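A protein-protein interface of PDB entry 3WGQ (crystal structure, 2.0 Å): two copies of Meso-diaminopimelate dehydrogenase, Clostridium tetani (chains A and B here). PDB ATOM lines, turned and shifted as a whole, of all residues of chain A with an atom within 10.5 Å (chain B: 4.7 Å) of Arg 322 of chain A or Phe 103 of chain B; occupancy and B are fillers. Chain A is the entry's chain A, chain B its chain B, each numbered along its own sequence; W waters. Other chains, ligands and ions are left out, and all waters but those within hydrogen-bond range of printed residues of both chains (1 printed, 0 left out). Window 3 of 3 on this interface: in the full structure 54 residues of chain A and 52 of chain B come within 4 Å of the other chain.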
ATOM      1  N   SER A 311     -27.915  27.631 -17.413  1.00  0.00           N
ATOM      2  CA  SER A 311     -26.823  28.379 -18.044  1.00  0.00           C
ATOM      3  C   SER A 311     -27.207  28.872 -19.441  1.00  0.00           C
ATOM      4  O   SER A 311     -26.678  29.871 -19.923  1.00  0.00           O
ATOM      5  CB  SER A 311     -25.569  27.504 -18.157  1.00  0.00           C
ATOM      6  OG  SER A 311     -25.824  26.352 -18.947  1.00  0.00           O
ATOM      7  N   SER A 314     -28.424  32.605 -19.858  1.00  0.00           N
ATOM      8  CA  SER A 314     -27.547  33.760 -19.715  1.00  0.00           C
ATOM      9  C   SER A 314     -26.585  34.005 -20.872  1.00  0.00           C
ATOM     10  O   SER A 314     -26.090  33.063 -21.486  1.00  0.00           O
ATOM     11  CB  SER A 314     -26.737  33.636 -18.421  1.00  0.00           C
ATOM     12  OG  SER A 314     -25.769  34.674 -18.336  1.00  0.00           O
ATOM     13  N   LYS A 316     -23.747  35.330 -20.510  1.00  0.00           N
ATOM     14  CA  LYS A 316     -22.399  35.236 -19.947  1.00  0.00           C
ATOM     15  C   LYS A 316     -21.803  33.884 -20.284  1.00  0.00           C
ATOM     16  O   LYS A 316     -22.526  32.948 -20.629  1.00  0.00           O
ATOM     17  CB  LYS A 316     -22.429  35.422 -18.420  1.00  0.00           C
ATOM     18  CG  LYS A 316     -22.758  36.844 -17.968  1.00  0.00           C
ATOM     19  CD  LYS A 316     -22.977  36.943 -16.454  1.00  0.00           C
ATOM     20  CE  LYS A 316     -23.289  38.386 -16.049  1.00  0.00           C
ATOM     21  NZ  LYS A 316     -23.646  38.561 -14.607  1.00  0.00           N
ATOM     22  N   THR A 317     -20.482  33.784 -20.179  1.00  0.00           N
ATOM     23  CA  THR A 317     -19.777  32.541 -20.476  1.00  0.00           C
ATOM     24  C   THR A 317     -19.853  31.601 -19.278  1.00  0.00           C
ATOM     25  O   THR A 317     -20.062  32.040 -18.149  1.00  0.00           O
ATOM     26  CB  THR A 317     -18.291  32.806 -20.790  1.00  0.00           C
ATOM     27  OG1 THR A 317     -17.639  33.318 -19.622  1.00  0.00           O
ATOM     28  CG2 THR A 317     -18.165  33.824 -21.905  1.00  0.00           C
ATOM     29  N   PRO A 318     -19.684  30.293 -19.510  1.00  0.00           N
ATOM     30  CA  PRO A 318     -19.740  29.321 -18.414  1.00  0.00           C
ATOM     31  C   PRO A 318     -18.753  29.662 -17.299  1.00  0.00           C
ATOM     32  O   PRO A 318     -19.033  29.447 -16.124  1.00  0.00           O
ATOM     33  CB  PRO A 318     -19.403  28.002 -19.106  1.00  0.00           C
ATOM     34  CG  PRO A 318     -19.977  28.202 -20.484  1.00  0.00           C
ATOM     35  CD  PRO A 318     -19.546  29.617 -20.812  1.00  0.00           C
ATOM     36  N   GLU A 319     -17.598  30.202 -17.675  1.00  0.00           N
ATOM     37  CA  GLU A 319     -16.581  30.574 -16.701  1.00  0.00           C
ATOM     38  C   GLU A 319     -17.024  31.761 -15.872  1.00  0.00           C
ATOM     39  O   GLU A 319     -16.790  31.799 -14.667  1.00  0.00           O
ATOM     40  CB  GLU A 319     -15.274  30.929 -17.402  1.00  0.00           C
ATOM     41  CG  GLU A 319     -14.579  29.749 -18.021  1.00  0.00           C
ATOM     42  CD  GLU A 319     -13.403  30.177 -18.854  1.00  0.00           C
ATOM     43  OE1 GLU A 319     -12.577  30.956 -18.332  1.00  0.00           O
ATOM     44  OE2 GLU A 319     -13.310  29.740 -20.023  1.00  0.00           O
ATOM     45  N   GLU A 320     -17.651  32.735 -16.524  1.00  0.00           N
ATOM     46  CA  GLU A 320     -18.122  33.924 -15.830  1.00  0.00           C
ATOM     47  C   GLU A 320     -19.170  33.549 -14.790  1.00  0.00           C
ATOM     48  O   GLU A 320     -19.169  34.076 -13.679  1.00  0.00           O
ATOM     49  CB  GLU A 320     -18.720  34.922 -16.819  1.00  0.00           C
ATOM     50  CG  GLU A 320     -17.699  35.567 -17.736  1.00  0.00           C
ATOM     51  CD  GLU A 320     -18.333  36.564 -18.687  1.00  0.00           C
ATOM     52  OE1 GLU A 320     -19.383  36.231 -19.280  1.00  0.00           O
ATOM     53  OE2 GLU A 320     -17.779  37.672 -18.846  1.00  0.00           O
ATOM     54  N   LEU A 321     -20.061  32.636 -15.161  1.00  0.00           N
ATOM     55  CA  LEU A 321     -21.112  32.190 -14.258  1.00  0.00           C
ATOM     56  C   LEU A 321     -20.539  31.455 -13.043  1.00  0.00           C
ATOM     57  O   LEU A 321     -20.950  31.709 -11.911  1.00  0.00           O
ATOM     58  CB  LEU A 321     -22.105  31.282 -15.003  1.00  0.00           C
ATOM     59  CG  LEU A 321     -22.878  31.872 -16.195  1.00  0.00           C
ATOM     60  CD1 LEU A 321     -23.841  30.827 -16.735  1.00  0.00           C
ATOM     61  CD2 LEU A 321     -23.640  33.120 -15.786  1.00  0.00           C
ATOM     62  N   ARG A 322     -19.595  30.544 -13.276  1.00  0.00           N
ATOM     63  CA  ARG A 322     -18.995  29.784 -12.183  1.00  0.00           C
ATOM     64  C   ARG A 322     -18.231  30.671 -11.220  1.00  0.00           C
ATOM     65  O   ARG A 322     -18.262  30.460 -10.009  1.00  0.00           O
ATOM     66  CB  ARG A 322     -18.034  28.722 -12.709  1.00  0.00           C
ATOM     67  CG  ARG A 322     -18.664  27.697 -13.615  1.00  0.00           C
ATOM     68  CD  ARG A 322     -17.814  26.438 -13.674  1.00  0.00           C
ATOM     69  NE  ARG A 322     -18.119  25.669 -14.869  1.00  0.00           N
ATOM     70  CZ  ARG A 322     -17.532  25.856 -16.045  1.00  0.00           C
ATOM     71  NH1 ARG A 322     -16.592  26.783 -16.188  1.00  0.00           N
ATOM     72  NH2 ARG A 322     -17.904  25.126 -17.083  1.00  0.00           N
ATOM     73  N   LYS A 323     -17.531  31.655 -11.768  1.00  0.00           N
ATOM     74  CA  LYS A 323     -16.756  32.568 -10.954  1.00  0.00           C
ATOM     75  C   LYS A 323     -17.656  33.532 -10.200  1.00  0.00           C
ATOM     76  O   LYS A 323     -17.388  33.874  -9.056  1.00  0.00           O
ATOM     77  CB  LYS A 323     -15.794  33.359 -11.838  1.00  0.00           C
ATOM     78  CG  LYS A 323     -14.916  34.347 -11.085  1.00  0.00           C
ATOM     79  CD  LYS A 323     -14.048  35.130 -12.055  1.00  0.00           C
ATOM     80  CE  LYS A 323     -13.095  36.055 -11.316  1.00  0.00           C
ATOM     81  NZ  LYS A 323     -13.822  37.035 -10.469  1.00  0.00           N
ATOM     82  N   GLU A 324     -18.736  33.957 -10.844  1.00  0.00           N
ATOM     83  CA  GLU A 324     -19.643  34.921 -10.239  1.00  0.00           C
ATOM     84  C   GLU A 324     -20.796  34.406  -9.379  1.00  0.00           C
ATOM     85  O   GLU A 324     -20.970  34.842  -8.245  1.00  0.00           O
ATOM     86  CB  GLU A 324     -20.256  35.808 -11.326  1.00  0.00           C
ATOM     87  CG  GLU A 324     -19.307  36.751 -12.024  1.00  0.00           C
ATOM     88  CD  GLU A 324     -19.991  37.491 -13.151  1.00  0.00           C
ATOM     89  OE1 GLU A 324     -21.121  37.991 -12.936  1.00  0.00           O
ATOM     90  OE2 GLU A 324     -19.400  37.575 -14.249  1.00  0.00           O
ATOM     91  N   LEU A 325     -21.583  33.487  -9.926  1.00  0.00           N
ATOM     92  CA  LEU A 325     -22.776  32.992  -9.243  1.00  0.00           C
ATOM     93  C   LEU A 325     -22.743  31.644  -8.544  1.00  0.00           C
ATOM     94  O   LEU A 325     -23.636  31.346  -7.744  1.00  0.00           O
ATOM     95  CB  LEU A 325     -23.935  32.951 -10.237  1.00  0.00           C
ATOM     96  CG  LEU A 325     -24.311  34.233 -10.965  1.00  0.00           C
ATOM     97  CD1 LEU A 325     -25.432  33.936 -11.937  1.00  0.00           C
ATOM     98  CD2 LEU A 325     -24.736  35.296  -9.959  1.00  0.00           C
ATOM     99  N   LEU A 326     -21.753  30.814  -8.845  1.00  0.00           N
ATOM    100  CA  LEU A 326     -21.721  29.496  -8.242  1.00  0.00           C
ATOM    101  C   LEU A 326     -21.383  29.505  -6.755  1.00  0.00           C
ATOM    102  O   LEU A 326     -20.252  29.892  -6.403  1.00  0.00           O
ATOM    103  CB  LEU A 326     -20.760  28.589  -9.020  1.00  0.00           C
ATOM    104  CG  LEU A 326     -20.892  27.084  -8.772  1.00  0.00           C
ATOM    105  CD1 LEU A 326     -22.359  26.666  -8.767  1.00  0.00           C
ATOM    106  CD2 LEU A 326     -20.117  26.336  -9.850  1.00  0.00           C
ATOM    107  OXT LEU A 326     -22.273  29.124  -5.955  1.00  0.00           O
ATOM    108  N   ILE B  99     -13.717  27.875  -6.439  1.00  0.00           N
ATOM    109  CA  ILE B  99     -14.482  27.003  -7.325  1.00  0.00           C
ATOM    110  C   ILE B  99     -13.884  26.905  -8.729  1.00  0.00           C
ATOM    111  O   ILE B  99     -13.781  25.817  -9.290  1.00  0.00           O
ATOM    112  CB  ILE B  99     -15.970  27.447  -7.414  1.00  0.00           C
ATOM    113  CG1 ILE B  99     -16.753  26.835  -6.247  1.00  0.00           C
ATOM    114  CG2 ILE B  99     -16.573  27.024  -8.752  1.00  0.00           C
ATOM    115  CD1 ILE B  99     -18.265  27.053  -6.307  1.00  0.00           C
ATOM    116  N   PRO B 100     -13.486  28.041  -9.321  1.00  0.00           N
ATOM    117  CA  PRO B 100     -12.905  27.984 -10.667  1.00  0.00           C
ATOM    118  C   PRO B 100     -11.708  27.038 -10.742  1.00  0.00           C
ATOM    119  O   PRO B 100     -11.509  26.347 -11.748  1.00  0.00           O
ATOM    120  CB  PRO B 100     -12.521  29.435 -10.929  1.00  0.00           C
ATOM    121  CG  PRO B 100     -13.614  30.183 -10.220  1.00  0.00           C
ATOM    122  CD  PRO B 100     -13.708  29.437  -8.905  1.00  0.00           C
ATOM    123  N   GLN B 101     -10.921  27.011  -9.669  1.00  0.00           N
ATOM    124  CA  GLN B 101      -9.734  26.162  -9.583  1.00  0.00           C
ATOM    125  C   GLN B 101     -10.122  24.693  -9.488  1.00  0.00           C
ATOM    126  O   GLN B 101      -9.579  23.845 -10.194  1.00  0.00           O
ATOM    127  CB  GLN B 101      -8.911  26.535  -8.345  1.00  0.00           C
ATOM    128  CG  GLN B 101      -7.661  25.684  -8.135  1.00  0.00           C
ATOM    129  CD  GLN B 101      -7.093  25.800  -6.725  1.00  0.00           C
ATOM    130  OE1 GLN B 101      -6.804  26.900  -6.242  1.00  0.00           O
ATOM    131  NE2 GLN B 101      -6.930  24.662  -6.062  1.00  0.00           N
ATOM    132  N   HIS B 102     -11.058  24.401  -8.593  1.00  0.00           N
ATOM    133  CA  HIS B 102     -11.519  23.037  -8.385  1.00  0.00           C
ATOM    134  C   HIS B 102     -12.130  22.492  -9.668  1.00  0.00           C
ATOM    135  O   HIS B 102     -11.979  21.313  -9.984  1.00  0.00           O
ATOM    136  CB  HIS B 102     -12.550  23.003  -7.252  1.00  0.00           C
ATOM    137  CG  HIS B 102     -13.047  21.630  -6.923  1.00  0.00           C
ATOM    138  ND1 HIS B 102     -12.230  20.641  -6.420  1.00  0.00           N
ATOM    139  CD2 HIS B 102     -14.281  21.082  -7.026  1.00  0.00           C
ATOM    140  CE1 HIS B 102     -12.939  19.543  -6.225  1.00  0.00           C
ATOM    141  NE2 HIS B 102     -14.187  19.784  -6.585  1.00  0.00           N
ATOM    142  N   PHE B 103     -12.820  23.356 -10.406  1.00  0.00           N
ATOM    143  CA  PHE B 103     -13.454  22.936 -11.648  1.00  0.00           C
ATOM    144  C   PHE B 103     -12.418  22.491 -12.665  1.00  0.00           C
ATOM    145  O   PHE B 103     -12.563  21.443 -13.288  1.00  0.00           O
ATOM    146  CB  PHE B 103     -14.280  24.064 -12.260  1.00  0.00           C
ATOM    147  CG  PHE B 103     -15.062  23.637 -13.472  1.00  0.00           C
ATOM    148  CD1 PHE B 103     -16.228  22.890 -13.335  1.00  0.00           C
ATOM    149  CD2 PHE B 103     -14.609  23.939 -14.751  1.00  0.00           C
ATOM    150  CE1 PHE B 103     -16.932  22.445 -14.457  1.00  0.00           C
ATOM    151  CE2 PHE B 103     -15.302  23.500 -15.880  1.00  0.00           C
ATOM    152  CZ  PHE B 103     -16.466  22.750 -15.732  1.00  0.00           C
ATOM    153  N   GLU B 104     -11.381  23.299 -12.838  1.00  0.00           N
ATOM    154  CA  GLU B 104     -10.322  22.980 -13.790  1.00  0.00           C
ATOM    155  C   GLU B 104      -9.636  21.670 -13.439  1.00  0.00           C
ATOM    156  O   GLU B 104      -9.471  20.803 -14.294  1.00  0.00           O
ATOM    157  CB  GLU B 104      -9.285  24.105 -13.834  1.00  0.00           C
ATOM    158  CG  GLU B 104      -9.803  25.391 -14.455  1.00  0.00           C
ATOM    159  CD  GLU B 104     -10.366  25.179 -15.852  1.00  0.00           C
ATOM    160  OE1 GLU B 104      -9.625  24.668 -16.719  1.00  0.00           O
ATOM    161  OE2 GLU B 104     -11.548  25.521 -16.082  1.00  0.00           O
ATOM    162  N   ARG B 105      -9.247  21.526 -12.177  1.00  0.00           N
ATOM    163  CA  ARG B 105      -8.577  20.313 -11.734  1.00  0.00           C
ATOM    164  C   ARG B 105      -9.451  19.084 -11.950  1.00  0.00           C
ATOM    165  O   ARG B 105      -8.983  18.065 -12.454  1.00  0.00           O
ATOM    166  CB  ARG B 105      -8.191  20.417 -10.252  1.00  0.00           C
ATOM    167  CG  ARG B 105      -7.406  19.210  -9.735  1.00  0.00           C
ATOM    168  CD  ARG B 105      -6.071  19.046 -10.473  1.00  0.00           C
ATOM    169  NE  ARG B 105      -5.438  17.743 -10.251  1.00  0.00           N
ATOM    170  CZ  ARG B 105      -5.004  17.297  -9.074  1.00  0.00           C
ATOM    171  NH1 ARG B 105      -5.128  18.045  -7.982  1.00  0.00           N
ATOM    172  NH2 ARG B 105      -4.441  16.097  -8.986  1.00  0.00           N
ATOM    173  N   MET B 106     -10.723  19.181 -11.569  1.00  0.00           N
ATOM    174  CA  MET B 106     -11.636  18.056 -11.726  1.00  0.00           C
ATOM    175  C   MET B 106     -11.975  17.768 -13.180  1.00  0.00           C
ATOM    176  O   MET B 106     -12.237  16.626 -13.539  1.00  0.00           O
ATOM    177  CB  MET B 106     -12.930  18.303 -10.944  1.00  0.00           C
ATOM    178  CG  MET B 106     -12.760  18.316  -9.435  1.00  0.00           C
ATOM    179  SD  MET B 106     -12.195  16.743  -8.784  1.00  0.00           S
ATOM    180  CE  MET B 106     -13.719  15.813  -8.689  1.00  0.00           C
ATOM    181  N   ASP B 107     -11.975  18.803 -14.014  1.00  0.00           N
ATOM    182  CA  ASP B 107     -12.295  18.642 -15.432  1.00  0.00           C
ATOM    183  C   ASP B 107     -11.207  17.824 -16.128  1.00  0.00           C
ATOM    184  O   ASP B 107     -11.481  16.781 -16.727  1.00  0.00           O
ATOM    185  CB  ASP B 107     -12.443  20.016 -16.097  1.00  0.00           C
ATOM    186  CG  ASP B 107     -13.041  19.934 -17.494  1.00  0.00           C
ATOM    187  OD1 ASP B 107     -13.948  19.101 -17.712  1.00  0.00           O
ATOM    188  OD2 ASP B 107     -12.617  20.713 -18.372  1.00  0.00           O
ATOM    189  N   ALA B 302     -15.998  17.801 -16.066  1.00  0.00           N
ATOM    190  CA  ALA B 302     -16.657  18.369 -14.904  1.00  0.00           C
ATOM    191  C   ALA B 302     -17.856  19.235 -15.299  1.00  0.00           C
ATOM    192  O   ALA B 302     -17.850  19.892 -16.337  1.00  0.00           O
ATOM    193  CB  ALA B 302     -15.662  19.195 -14.103  1.00  0.00           C
ATOM    194  N   VAL B 303     -18.884  19.210 -14.459  1.00  0.00           N
ATOM    195  CA  VAL B 303     -20.092  19.997 -14.676  1.00  0.00           C
ATOM    196  C   VAL B 303     -20.548  20.572 -13.343  1.00  0.00           C
ATOM    197  O   VAL B 303     -20.113  20.118 -12.279  1.00  0.00           O
ATOM    198  CB  VAL B 303     -21.251  19.143 -15.247  1.00  0.00           C
ATOM    199  CG1 VAL B 303     -20.955  18.757 -16.680  1.00  0.00           C
ATOM    200  CG2 VAL B 303     -21.463  17.900 -14.386  1.00  0.00           C
ATOM    201  N   THR B 304     -21.418  21.576 -13.410  1.00  0.00           N
ATOM    202  CA  THR B 304     -21.972  22.194 -12.214  1.00  0.00           C
ATOM    203  C   THR B 304     -23.496  22.104 -12.316  1.00  0.00           C
ATOM    204  O   THR B 304     -24.029  21.704 -13.354  1.00  0.00           O
ATOM    205  CB  THR B 304     -21.562  23.684 -12.094  1.00  0.00           C
ATOM    206  OG1 THR B 304     -22.246  24.456 -13.087  1.00  0.00           O
ATOM    207  CG2 THR B 304     -20.055  23.840 -12.281  1.00  0.00           C
ATOM    208  N   LEU B 306     -25.431  24.287 -12.825  1.00  0.00           N
ATOM    209  CA  LEU B 306     -25.854  25.209 -13.874  1.00  0.00           C
ATOM    210  C   LEU B 306     -25.930  24.556 -15.253  1.00  0.00           C
ATOM    211  O   LEU B 306     -26.579  25.084 -16.147  1.00  0.00           O
ATOM    212  CB  LEU B 306     -24.900  26.408 -13.955  1.00  0.00           C
ATOM    213  CG  LEU B 306     -24.499  27.135 -12.662  1.00  0.00           C
ATOM    214  CD1 LEU B 306     -23.561  28.286 -13.005  1.00  0.00           C
ATOM    215  CD2 LEU B 306     -25.728  27.650 -11.947  1.00  0.00           C
HETATM  216  O   HOH W   1     -20.920  24.962 -15.262  1.00  0.00           O
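O of Leu 306 of chain B lies within hydrogen-bond range of N of Ser 311 of chain A, 3.1 Å away.
The backbone NH (N) of Leu 326 of chain A is in hydrogen-bond range of the backbone carbonyl oxygen (O) of Leu 321 of chain A (3.3 Å).
The side-chain hydroxyl of Thr 304 of chain B sits close to the backbone NH of Leu 306 of chain B (3.2 Å).
Among the printed residues, merely in contact across the chains: Arg 322 of chain A with Phe 103 of chain B, Leu 326 of chain A with Ile 99 of chain B, Leu 326 of chain A with Thr 304 of chain B, Arg 322 of chain A with Thr 304 of chain B and Leu 321 of chain A with Leu 306 of chain B.
Of the printed residues of chain B, Ser 311 of chain A touches Leu 306.
Of the printed residues of chain B, Leu 321 of chain A touches Leu 306 (3.9 Å).
Of chain B, only Phe 103 and Thr 304 come within 4 Å of Arg 322 of chain A.
Of the printed residues of chain B, Leu 326 of chain A touches Ile 99 and Thr 304.
Of the printed residues of chain A, Ile 99 of chain B touches Leu 326.
Phe 103 of chain B touches just one residue of chain A: Arg 322 (3.1 Å).
No residue of chain A comes within 4 Å of Asp 107 of chain B.
Printed residues of chain A within 4 Å of Thr 304 of chain B: Arg 322 and Leu 326.
Printed residues of chain A within 4 Å of Leu 306 of chain B: Ser 311 (3.1 Å) and Leu 321 (3.9 Å).
The nearest residue of chain A that does not touch Phe 103 of chain B is Leu 326 of chain A (6.3 Å).
Of the 13 printed residues of chain A, 4 touch a printed residue of chain B.
Printed residues of chain A that touch a printed residue of chain B: Ser 311, Leu 321, Arg 322 and Leu 326.
Along chain B the printed residues that touch a printed residue of chain A span positions 99 to 306.
Among the printed residues, no Asp or Glu carboxylate lies within 4 Å of a Lys or Arg side-chain nitrogen of the other chain.
No position is printed for both chains.
Water W1 bridges OG1 of Thr 304 of chain B (2.6 Å) and NE of Arg 322 of chain A (2.9 Å).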
